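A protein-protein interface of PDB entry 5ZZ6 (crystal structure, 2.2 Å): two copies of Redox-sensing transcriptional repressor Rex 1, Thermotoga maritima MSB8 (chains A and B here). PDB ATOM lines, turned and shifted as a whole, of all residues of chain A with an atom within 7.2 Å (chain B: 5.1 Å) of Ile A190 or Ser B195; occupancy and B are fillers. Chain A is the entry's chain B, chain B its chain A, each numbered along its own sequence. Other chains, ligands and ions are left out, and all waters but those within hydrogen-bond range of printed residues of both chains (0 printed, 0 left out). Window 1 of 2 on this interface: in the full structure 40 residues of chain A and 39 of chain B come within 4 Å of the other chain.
N of Ile A190 lies within hydrogen-bond range of O of Asn A175 (2.8 Å). The backbone NH of Ile A151 sits at hydrogen-bond distance from the backbone carbonyl oxygen of Leu A174 (2.8 Å). The backbone NH of Glu A188 lies within hydrogen-bond range of the backbone carbonyl oxygen of Ile A173, at 2.8 Å. O of Asp B191 is in hydrogen-bond range of OG of Ser B195, 2.9 Å away. OD1 of Asp B191 is in hydrogen-bond range of N of Thr B193 (3.2 Å). OG of Ser A195 lies within hydrogen-bond range of O of Asp A191.
Among the printed residues, pairs that only touch across the chains: Ile A173 with Leu B199 (3.5 Å), Glu A188 with Ser B195 (3.5 Å), Phe A108 with Arg B197 (3.5 Å), Ile A190 with Ser B195 (3.5 Å), Leu A174 with Leu B196 (3.6 Å), Leu A174 with Leu B199 (3.6 Å), Phe A108 with Leu B196 (3.7 Å), Ile A192 with Ile B190 (3.7 Å), Glu A188 with Leu B199 (3.7 Å), Ile A190 with Ile B190 (3.7 Å), Glu A188 with Val B198 (3.8 Å), Phe A108 with Thr B193 (3.8 Å), Ser A195 with Ile B190 (3.8 Å) and Ile A190 with Ile B192 (3.9 Å).
Of the printed residues of chain B, Leu A174 touches Leu B196 (3.6 Å) and Leu B199 (3.6 Å). Ala A194 touches none of the printed residues of chain B. Of the printed residues of chain A, Ile B192 touches Ile A190. Ala B194 touches none of the printed residues of chain A. Of chain A, only Glu A188 and Ile A190 come within 4 Å of Ser B195. Printed residues of chain A within 4 Å of Leu B196: Phe A108 and Leu A174. The nearest residue of chain B that does not touch Ile A190 is Asp B191 (4.6 Å).
Printed residues of chain A that touch a printed residue of chain B: Phe A108, Ile A173, Leu A174, Glu A188, Ile A190, Ile A192 and Ser A195. Hydrophobic or aromatic side chains of chain A that line the printed part of chain B: Phe A108, Leu A174, Ile A190 and Ile A192. Along chain A the printed residues that touch a printed residue of chain B span positions 108 to 195. Among the printed residues, 14 pairs touch across the chains. Among the printed residues, no Asp or Glu carboxylate lies within 4 Å of a Lys or Arg side-chain nitrogen of the other chain.
Ile A190 touches its own counterpart, Ile B190. Ile A190 touches Ile B192, and with the chains exchanged Ile A192 touches Ile B190. Ile A190 touches Ser B195, and with the chains exchanged Ser A195 touches Ile B190. Positions printed for both chains: 190, 191, 192, 193, 194 and 195.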
ATOM      1  N   ILE A  93       8.737  18.882 -20.720  1.00  0.00           N
ATOM      2  CA  ILE A  93       8.541  20.119 -21.470  1.00  0.00           C
ATOM      3  C   ILE A  93       8.387  21.299 -20.521  1.00  0.00           C
ATOM      4  O   ILE A  93       9.060  22.328 -20.666  1.00  0.00           O
ATOM      5  CB  ILE A  93       7.325  19.992 -22.404  1.00  0.00           C
ATOM      6  CG1 ILE A  93       7.617  19.004 -23.531  1.00  0.00           C
ATOM      7  CG2 ILE A  93       6.950  21.356 -22.966  1.00  0.00           C
ATOM      8  CD1 ILE A  93       8.753  19.440 -24.428  1.00  0.00           C
ATOM      9  N   PHE A 108       9.294  37.311 -22.151  1.00  0.00           N
ATOM     10  CA  PHE A 108       8.308  36.357 -21.662  1.00  0.00           C
ATOM     11  C   PHE A 108       8.734  35.868 -20.286  1.00  0.00           C
ATOM     12  O   PHE A 108       9.820  35.296 -20.135  1.00  0.00           O
ATOM     13  CB  PHE A 108       8.150  35.189 -22.637  1.00  0.00           C
ATOM     14  CG  PHE A 108       7.786  35.607 -24.038  1.00  0.00           C
ATOM     15  CD1 PHE A 108       6.470  35.880 -24.377  1.00  0.00           C
ATOM     16  CD2 PHE A 108       8.761  35.723 -25.016  1.00  0.00           C
ATOM     17  CE1 PHE A 108       6.130  36.261 -25.667  1.00  0.00           C
ATOM     18  CE2 PHE A 108       8.433  36.111 -26.310  1.00  0.00           C
ATOM     19  CZ  PHE A 108       7.114  36.378 -26.633  1.00  0.00           C
ATOM     20  N   ILE A 151       0.627  24.971 -22.434  1.00  0.00           N
ATOM     21  CA  ILE A 151       0.082  23.651 -22.125  1.00  0.00           C
ATOM     22  C   ILE A 151       1.177  22.616 -22.359  1.00  0.00           C
ATOM     23  O   ILE A 151       1.556  22.338 -23.502  1.00  0.00           O
ATOM     24  CB  ILE A 151      -1.165  23.339 -22.962  1.00  0.00           C
ATOM     25  CG1 ILE A 151      -2.319  24.258 -22.563  1.00  0.00           C
ATOM     26  CG2 ILE A 151      -1.580  21.880 -22.784  1.00  0.00           C
ATOM     27  CD1 ILE A 151      -3.638  23.884 -23.214  1.00  0.00           C
ATOM     28  N   ILE A 173      -2.706  30.746 -25.932  1.00  0.00           N
ATOM     29  CA  ILE A 173      -2.220  29.445 -25.486  1.00  0.00           C
ATOM     30  C   ILE A 173      -1.109  28.976 -26.413  1.00  0.00           C
ATOM     31  O   ILE A 173      -1.303  28.895 -27.629  1.00  0.00           O
ATOM     32  CB  ILE A 173      -3.340  28.397 -25.424  1.00  0.00           C
ATOM     33  CG1 ILE A 173      -4.313  28.722 -24.285  1.00  0.00           C
ATOM     34  CG2 ILE A 173      -2.744  27.006 -25.232  1.00  0.00           C
ATOM     35  CD1 ILE A 173      -5.454  27.732 -24.167  1.00  0.00           C
ATOM     36  N   LEU A 174       0.052  28.679 -25.838  1.00  0.00           N
ATOM     37  CA  LEU A 174       1.091  27.914 -26.509  1.00  0.00           C
ATOM     38  C   LEU A 174       0.917  26.454 -26.109  1.00  0.00           C
ATOM     39  O   LEU A 174       1.055  26.111 -24.933  1.00  0.00           O
ATOM     40  CB  LEU A 174       2.479  28.416 -26.128  1.00  0.00           C
ATOM     41  CG  LEU A 174       3.639  27.650 -26.766  1.00  0.00           C
ATOM     42  CD1 LEU A 174       3.639  27.852 -28.269  1.00  0.00           C
ATOM     43  CD2 LEU A 174       4.961  28.064 -26.156  1.00  0.00           C
ATOM     44  N   ASN A 175       0.613  25.604 -27.080  1.00  0.00           N
ATOM     45  CA  ASN A 175       0.222  24.222 -26.834  1.00  0.00           C
ATOM     46  C   ASN A 175       1.316  23.286 -27.336  1.00  0.00           C
ATOM     47  O   ASN A 175       1.600  23.247 -28.537  1.00  0.00           O
ATOM     48  CB  ASN A 175      -1.110  23.918 -27.523  1.00  0.00           C
ATOM     49  CG  ASN A 175      -1.501  22.461 -27.426  1.00  0.00           C
ATOM     50  OD1 ASN A 175      -1.376  21.838 -26.374  1.00  0.00           O
ATOM     51  ND2 ASN A 175      -1.975  21.906 -28.533  1.00  0.00           N
ATOM     52  N   PHE A 176       1.928  22.544 -26.415  1.00  0.00           N
ATOM     53  CA  PHE A 176       2.896  21.510 -26.764  1.00  0.00           C
ATOM     54  C   PHE A 176       2.259  20.149 -26.977  1.00  0.00           C
ATOM     55  O   PHE A 176       2.907  19.259 -27.542  1.00  0.00           O
ATOM     56  CB  PHE A 176       3.957  21.365 -25.668  1.00  0.00           C
ATOM     57  CG  PHE A 176       5.047  22.381 -25.749  1.00  0.00           C
ATOM     58  CD1 PHE A 176       6.154  22.165 -26.550  1.00  0.00           C
ATOM     59  CD2 PHE A 176       4.973  23.545 -25.012  1.00  0.00           C
ATOM     60  CE1 PHE A 176       7.167  23.099 -26.621  1.00  0.00           C
ATOM     61  CE2 PHE A 176       5.979  24.485 -25.077  1.00  0.00           C
ATOM     62  CZ  PHE A 176       7.079  24.262 -25.885  1.00  0.00           C
ATOM     63  N   ALA A 177       1.026  19.961 -26.521  1.00  0.00           N
ATOM     64  CA  ALA A 177       0.396  18.656 -26.620  1.00  0.00           C
ATOM     65  C   ALA A 177      -0.068  18.408 -28.054  1.00  0.00           C
ATOM     66  O   ALA A 177      -0.655  19.295 -28.678  1.00  0.00           O
ATOM     67  CB  ALA A 177      -0.785  18.563 -25.657  1.00  0.00           C
ATOM     68  N   PRO A 178       0.199  17.195 -28.617  1.00  0.00           N
ATOM     69  CA  PRO A 178      -0.143  16.909 -30.026  1.00  0.00           C
ATOM     70  C   PRO A 178      -1.637  16.706 -30.236  1.00  0.00           C
ATOM     71  O   PRO A 178      -2.109  15.612 -30.564  1.00  0.00           O
ATOM     72  CB  PRO A 178       0.663  15.636 -30.305  1.00  0.00           C
ATOM     73  CG  PRO A 178       0.762  14.962 -28.986  1.00  0.00           C
ATOM     74  CD  PRO A 178       0.882  16.060 -27.969  1.00  0.00           C
ATOM     75  N   VAL A 187      -4.337  29.984 -30.342  1.00  0.00           N
ATOM     76  CA  VAL A 187      -3.508  28.861 -29.923  1.00  0.00           C
ATOM     77  C   VAL A 187      -2.368  28.716 -30.921  1.00  0.00           C
ATOM     78  O   VAL A 187      -2.607  28.605 -32.129  1.00  0.00           O
ATOM     79  CB  VAL A 187      -4.310  27.551 -29.833  1.00  0.00           C
ATOM     80  CG1 VAL A 187      -3.393  26.395 -29.458  1.00  0.00           C
ATOM     81  CG2 VAL A 187      -5.451  27.678 -28.823  1.00  0.00           C
ATOM     82  N   GLU A 188      -1.136  28.729 -30.424  1.00  0.00           N
ATOM     83  CA  GLU A 188       0.035  28.345 -31.204  1.00  0.00           C
ATOM     84  C   GLU A 188       0.435  26.937 -30.782  1.00  0.00           C
ATOM     85  O   GLU A 188       0.740  26.700 -29.610  1.00  0.00           O
ATOM     86  CB  GLU A 188       1.210  29.302 -30.988  1.00  0.00           C
ATOM     87  CG  GLU A 188       1.366  30.420 -32.010  1.00  0.00           C
ATOM     88  CD  GLU A 188       1.464  29.919 -33.447  1.00  0.00           C
ATOM     89  OE1 GLU A 188       0.471  30.064 -34.189  1.00  0.00           O
ATOM     90  OE2 GLU A 188       2.530  29.383 -33.830  1.00  0.00           O
ATOM     91  N   ASN A 189       0.424  26.007 -31.727  1.00  0.00           N
ATOM     92  CA  ASN A 189       0.876  24.656 -31.449  1.00  0.00           C
ATOM     93  C   ASN A 189       2.370  24.552 -31.697  1.00  0.00           C
ATOM     94  O   ASN A 189       2.905  25.157 -32.629  1.00  0.00           O
ATOM     95  CB  ASN A 189       0.135  23.637 -32.311  1.00  0.00           C
ATOM     96  CG  ASN A 189      -1.357  23.669 -32.086  1.00  0.00           C
ATOM     97  OD1 ASN A 189      -1.824  23.719 -30.950  1.00  0.00           O
ATOM     98  ND2 ASN A 189      -2.116  23.657 -33.174  1.00  0.00           N
ATOM     99  N   ILE A 190       3.044  23.803 -30.836  1.00  0.00           N
ATOM    100  CA  ILE A 190       4.400  23.336 -31.088  1.00  0.00           C
ATOM    101  C   ILE A 190       4.346  21.824 -30.996  1.00  0.00           C
ATOM    102  O   ILE A 190       4.130  21.268 -29.914  1.00  0.00           O
ATOM    103  CB  ILE A 190       5.423  23.918 -30.107  1.00  0.00           C
ATOM    104  CG1 ILE A 190       5.653  25.401 -30.404  1.00  0.00           C
ATOM    105  CG2 ILE A 190       6.732  23.157 -30.211  1.00  0.00           C
ATOM    106  CD1 ILE A 190       6.818  25.989 -29.644  1.00  0.00           C
ATOM    107  N   ASP A 191       4.502  21.159 -32.131  1.00  0.00           N
ATOM    108  CA  ASP A 191       4.396  19.706 -32.208  1.00  0.00           C
ATOM    109  C   ASP A 191       5.740  19.185 -32.701  1.00  0.00           C
ATOM    110  O   ASP A 191       6.037  19.247 -33.899  1.00  0.00           O
ATOM    111  CB  ASP A 191       3.247  19.299 -33.122  1.00  0.00           C
ATOM    112  CG  ASP A 191       2.964  17.812 -33.082  1.00  0.00           C
ATOM    113  OD1 ASP A 191       3.793  17.051 -32.537  1.00  0.00           O
ATOM    114  OD2 ASP A 191       1.909  17.406 -33.611  1.00  0.00           O
ATOM    115  N   ILE A 192       6.548  18.682 -31.768  1.00  0.00           N
ATOM    116  CA  ILE A 192       7.884  18.209 -32.112  1.00  0.00           C
ATOM    117  C   ILE A 192       7.806  17.052 -33.100  1.00  0.00           C
ATOM    118  O   ILE A 192       8.564  17.000 -34.075  1.00  0.00           O
ATOM    119  CB  ILE A 192       8.654  17.830 -30.834  1.00  0.00           C
ATOM    120  CG1 ILE A 192       8.948  19.091 -30.017  1.00  0.00           C
ATOM    121  CG2 ILE A 192       9.942  17.104 -31.175  1.00  0.00           C
ATOM    122  CD1 ILE A 192       9.291  18.834 -28.567  1.00  0.00           C
ATOM    123  N   THR A 193       6.876  16.118 -32.877  1.00  0.00           N
ATOM    124  CA  THR A 193       6.719  15.000 -33.799  1.00  0.00           C
ATOM    125  C   THR A 193       6.291  15.483 -35.180  1.00  0.00           C
ATOM    126  O   THR A 193       6.839  15.040 -36.198  1.00  0.00           O
ATOM    127  CB  THR A 193       5.710  13.992 -33.248  1.00  0.00           C
ATOM    128  OG1 THR A 193       6.152  13.529 -31.965  1.00  0.00           O
ATOM    129  CG2 THR A 193       5.577  12.804 -34.191  1.00  0.00           C
ATOM    130  N   ALA A 194       5.314  16.393 -35.237  1.00  0.00           N
ATOM    131  CA  ALA A 194       4.925  16.974 -36.516  1.00  0.00           C
ATOM    132  C   ALA A 194       6.108  17.654 -37.195  1.00  0.00           C
ATOM    133  O   ALA A 194       6.268  17.561 -38.416  1.00  0.00           O
ATOM    134  CB  ALA A 194       3.781  17.968 -36.329  1.00  0.00           C
ATOM    135  N   SER A 195       6.953  18.335 -36.419  1.00  0.00           N
ATOM    136  CA  SER A 195       8.113  18.993 -37.012  1.00  0.00           C
ATOM    137  C   SER A 195       9.118  17.972 -37.533  1.00  0.00           C
ATOM    138  O   SER A 195       9.766  18.196 -38.564  1.00  0.00           O
ATOM    139  CB  SER A 195       8.760  19.930 -35.997  1.00  0.00           C
ATOM    140  OG  SER A 195       8.020  21.132 -35.878  1.00  0.00           O
ATOM    141  N   ILE B 190      12.329  24.642 -34.451  1.00  0.00           N
ATOM    142  CA  ILE B 190      11.374  24.818 -33.371  1.00  0.00           C
ATOM    143  C   ILE B 190      11.897  25.946 -32.500  1.00  0.00           C
ATOM    144  O   ILE B 190      12.760  25.739 -31.637  1.00  0.00           O
ATOM    145  CB  ILE B 190      11.172  23.530 -32.554  1.00  0.00           C
ATOM    146  CG1 ILE B 190      10.606  22.421 -33.431  1.00  0.00           C
ATOM    147  CG2 ILE B 190      10.226  23.798 -31.404  1.00  0.00           C
ATOM    148  CD1 ILE B 190      10.423  21.116 -32.704  1.00  0.00           C
ATOM    149  N   ASP B 191      11.401  27.151 -32.742  1.00  0.00           N
ATOM    150  CA  ASP B 191      11.788  28.330 -31.977  1.00  0.00           C
ATOM    151  C   ASP B 191      10.642  28.640 -31.021  1.00  0.00           C
ATOM    152  O   ASP B 191       9.625  29.213 -31.418  1.00  0.00           O
ATOM    153  CB  ASP B 191      12.094  29.501 -32.904  1.00  0.00           C
ATOM    154  CG  ASP B 191      12.766  30.657 -32.181  1.00  0.00           C
ATOM    155  OD1 ASP B 191      12.548  30.816 -30.963  1.00  0.00           O
ATOM    156  OD2 ASP B 191      13.508  31.413 -32.839  1.00  0.00           O
ATOM    157  N   ILE B 192      10.816  28.252 -29.757  1.00  0.00           N
ATOM    158  CA  ILE B 192       9.769  28.447 -28.755  1.00  0.00           C
ATOM    159  C   ILE B 192       9.472  29.929 -28.574  1.00  0.00           C
ATOM    160  O   ILE B 192       8.309  30.344 -28.529  1.00  0.00           O
ATOM    161  CB  ILE B 192      10.183  27.780 -27.432  1.00  0.00           C
ATOM    162  CG1 ILE B 192      10.245  26.264 -27.622  1.00  0.00           C
ATOM    163  CG2 ILE B 192       9.226  28.161 -26.310  1.00  0.00           C
ATOM    164  CD1 ILE B 192      11.003  25.542 -26.542  1.00  0.00           C
ATOM    165  N   THR B 193      10.517  30.751 -28.482  1.00  0.00           N
ATOM    166  CA  THR B 193      10.313  32.184 -28.321  1.00  0.00           C
ATOM    167  C   THR B 193       9.596  32.779 -29.530  1.00  0.00           C
ATOM    168  O   THR B 193       8.653  33.563 -29.373  1.00  0.00           O
ATOM    169  CB  THR B 193      11.657  32.872 -28.077  1.00  0.00           C
ATOM    170  OG1 THR B 193      12.325  32.227 -26.984  1.00  0.00           O
ATOM    171  CG2 THR B 193      11.454  34.337 -27.732  1.00  0.00           C
ATOM    172  N   ALA B 194      10.009  32.399 -30.743  1.00  0.00           N
ATOM    173  CA  ALA B 194       9.330  32.897 -31.937  1.00  0.00           C
ATOM    174  C   ALA B 194       7.871  32.457 -31.969  1.00  0.00           C
ATOM    175  O   ALA B 194       6.988  33.234 -32.344  1.00  0.00           O
ATOM    176  CB  ALA B 194      10.056  32.430 -33.198  1.00  0.00           C
ATOM    177  N   SER B 195       7.602  31.209 -31.581  1.00  0.00           N
ATOM    178  CA  SER B 195       6.224  30.733 -31.508  1.00  0.00           C
ATOM    179  C   SER B 195       5.421  31.527 -30.487  1.00  0.00           C
ATOM    180  O   SER B 195       4.242  31.825 -30.705  1.00  0.00           O
ATOM    181  CB  SER B 195       6.208  29.244 -31.159  1.00  0.00           C
ATOM    182  OG  SER B 195       6.890  28.490 -32.145  1.00  0.00           O
ATOM    183  N   LEU B 196       6.040  31.860 -29.353  1.00  0.00           N
ATOM    184  CA  LEU B 196       5.397  32.758 -28.404  1.00  0.00           C
ATOM    185  C   LEU B 196       5.189  34.135 -29.017  1.00  0.00           C
ATOM    186  O   LEU B 196       4.144  34.764 -28.810  1.00  0.00           O
ATOM    187  CB  LEU B 196       6.234  32.850 -27.129  1.00  0.00           C
ATOM    188  CG  LEU B 196       6.087  31.609 -26.250  1.00  0.00           C
ATOM    189  CD1 LEU B 196       7.201  31.529 -25.223  1.00  0.00           C
ATOM    190  CD2 LEU B 196       4.729  31.643 -25.573  1.00  0.00           C
ATOM    191  N   ARG B 197       6.168  34.610 -29.794  1.00  0.00           N
ATOM    192  CA  ARG B 197       6.033  35.901 -30.459  1.00  0.00           C
ATOM    193  C   ARG B 197       4.887  35.883 -31.466  1.00  0.00           C
ATOM    194  O   ARG B 197       4.062  36.802 -31.501  1.00  0.00           O
ATOM    195  CB  ARG B 197       7.348  36.272 -31.150  1.00  0.00           C
ATOM    196  CG  ARG B 197       7.343  37.665 -31.761  1.00  0.00           C
ATOM    197  CD  ARG B 197       7.086  38.715 -30.689  1.00  0.00           C
ATOM    198  NE  ARG B 197       8.198  38.760 -29.742  1.00  0.00           N
ATOM    199  CZ  ARG B 197       8.117  39.227 -28.503  1.00  0.00           C
ATOM    200  NH1 ARG B 197       6.963  39.687 -28.032  1.00  0.00           N
ATOM    201  NH2 ARG B 197       9.195  39.221 -27.734  1.00  0.00           N
ATOM    202  N   VAL B 198       4.828  34.841 -32.298  1.00  0.00           N
ATOM    203  CA  VAL B 198       3.729  34.702 -33.252  1.00  0.00           C
ATOM    204  C   VAL B 198       2.390  34.701 -32.523  1.00  0.00           C
ATOM    205  O   VAL B 198       1.431  35.351 -32.957  1.00  0.00           O
ATOM    206  CB  VAL B 198       3.917  33.430 -34.103  1.00  0.00           C
ATOM    207  CG1 VAL B 198       2.679  33.158 -34.951  1.00  0.00           C
ATOM    208  CG2 VAL B 198       5.156  33.561 -34.993  1.00  0.00           C
ATOM    209  N   LEU B 199       2.307  33.982 -31.399  1.00  0.00           N
ATOM    210  CA  LEU B 199       1.081  33.982 -30.605  1.00  0.00           C
ATOM    211  C   LEU B 199       0.715  35.390 -30.150  1.00  0.00           C
ATOM    212  O   LEU B 199      -0.444  35.803 -30.259  1.00  0.00           O
ATOM    213  CB  LEU B 199       1.236  33.060 -29.392  1.00  0.00           C
ATOM    214  CG  LEU B 199       0.016  32.949 -28.464  1.00  0.00           C
ATOM    215  CD1 LEU B 199      -1.217  32.485 -29.231  1.00  0.00           C
ATOM    216  CD2 LEU B 199       0.300  32.005 -27.284  1.00  0.00           C
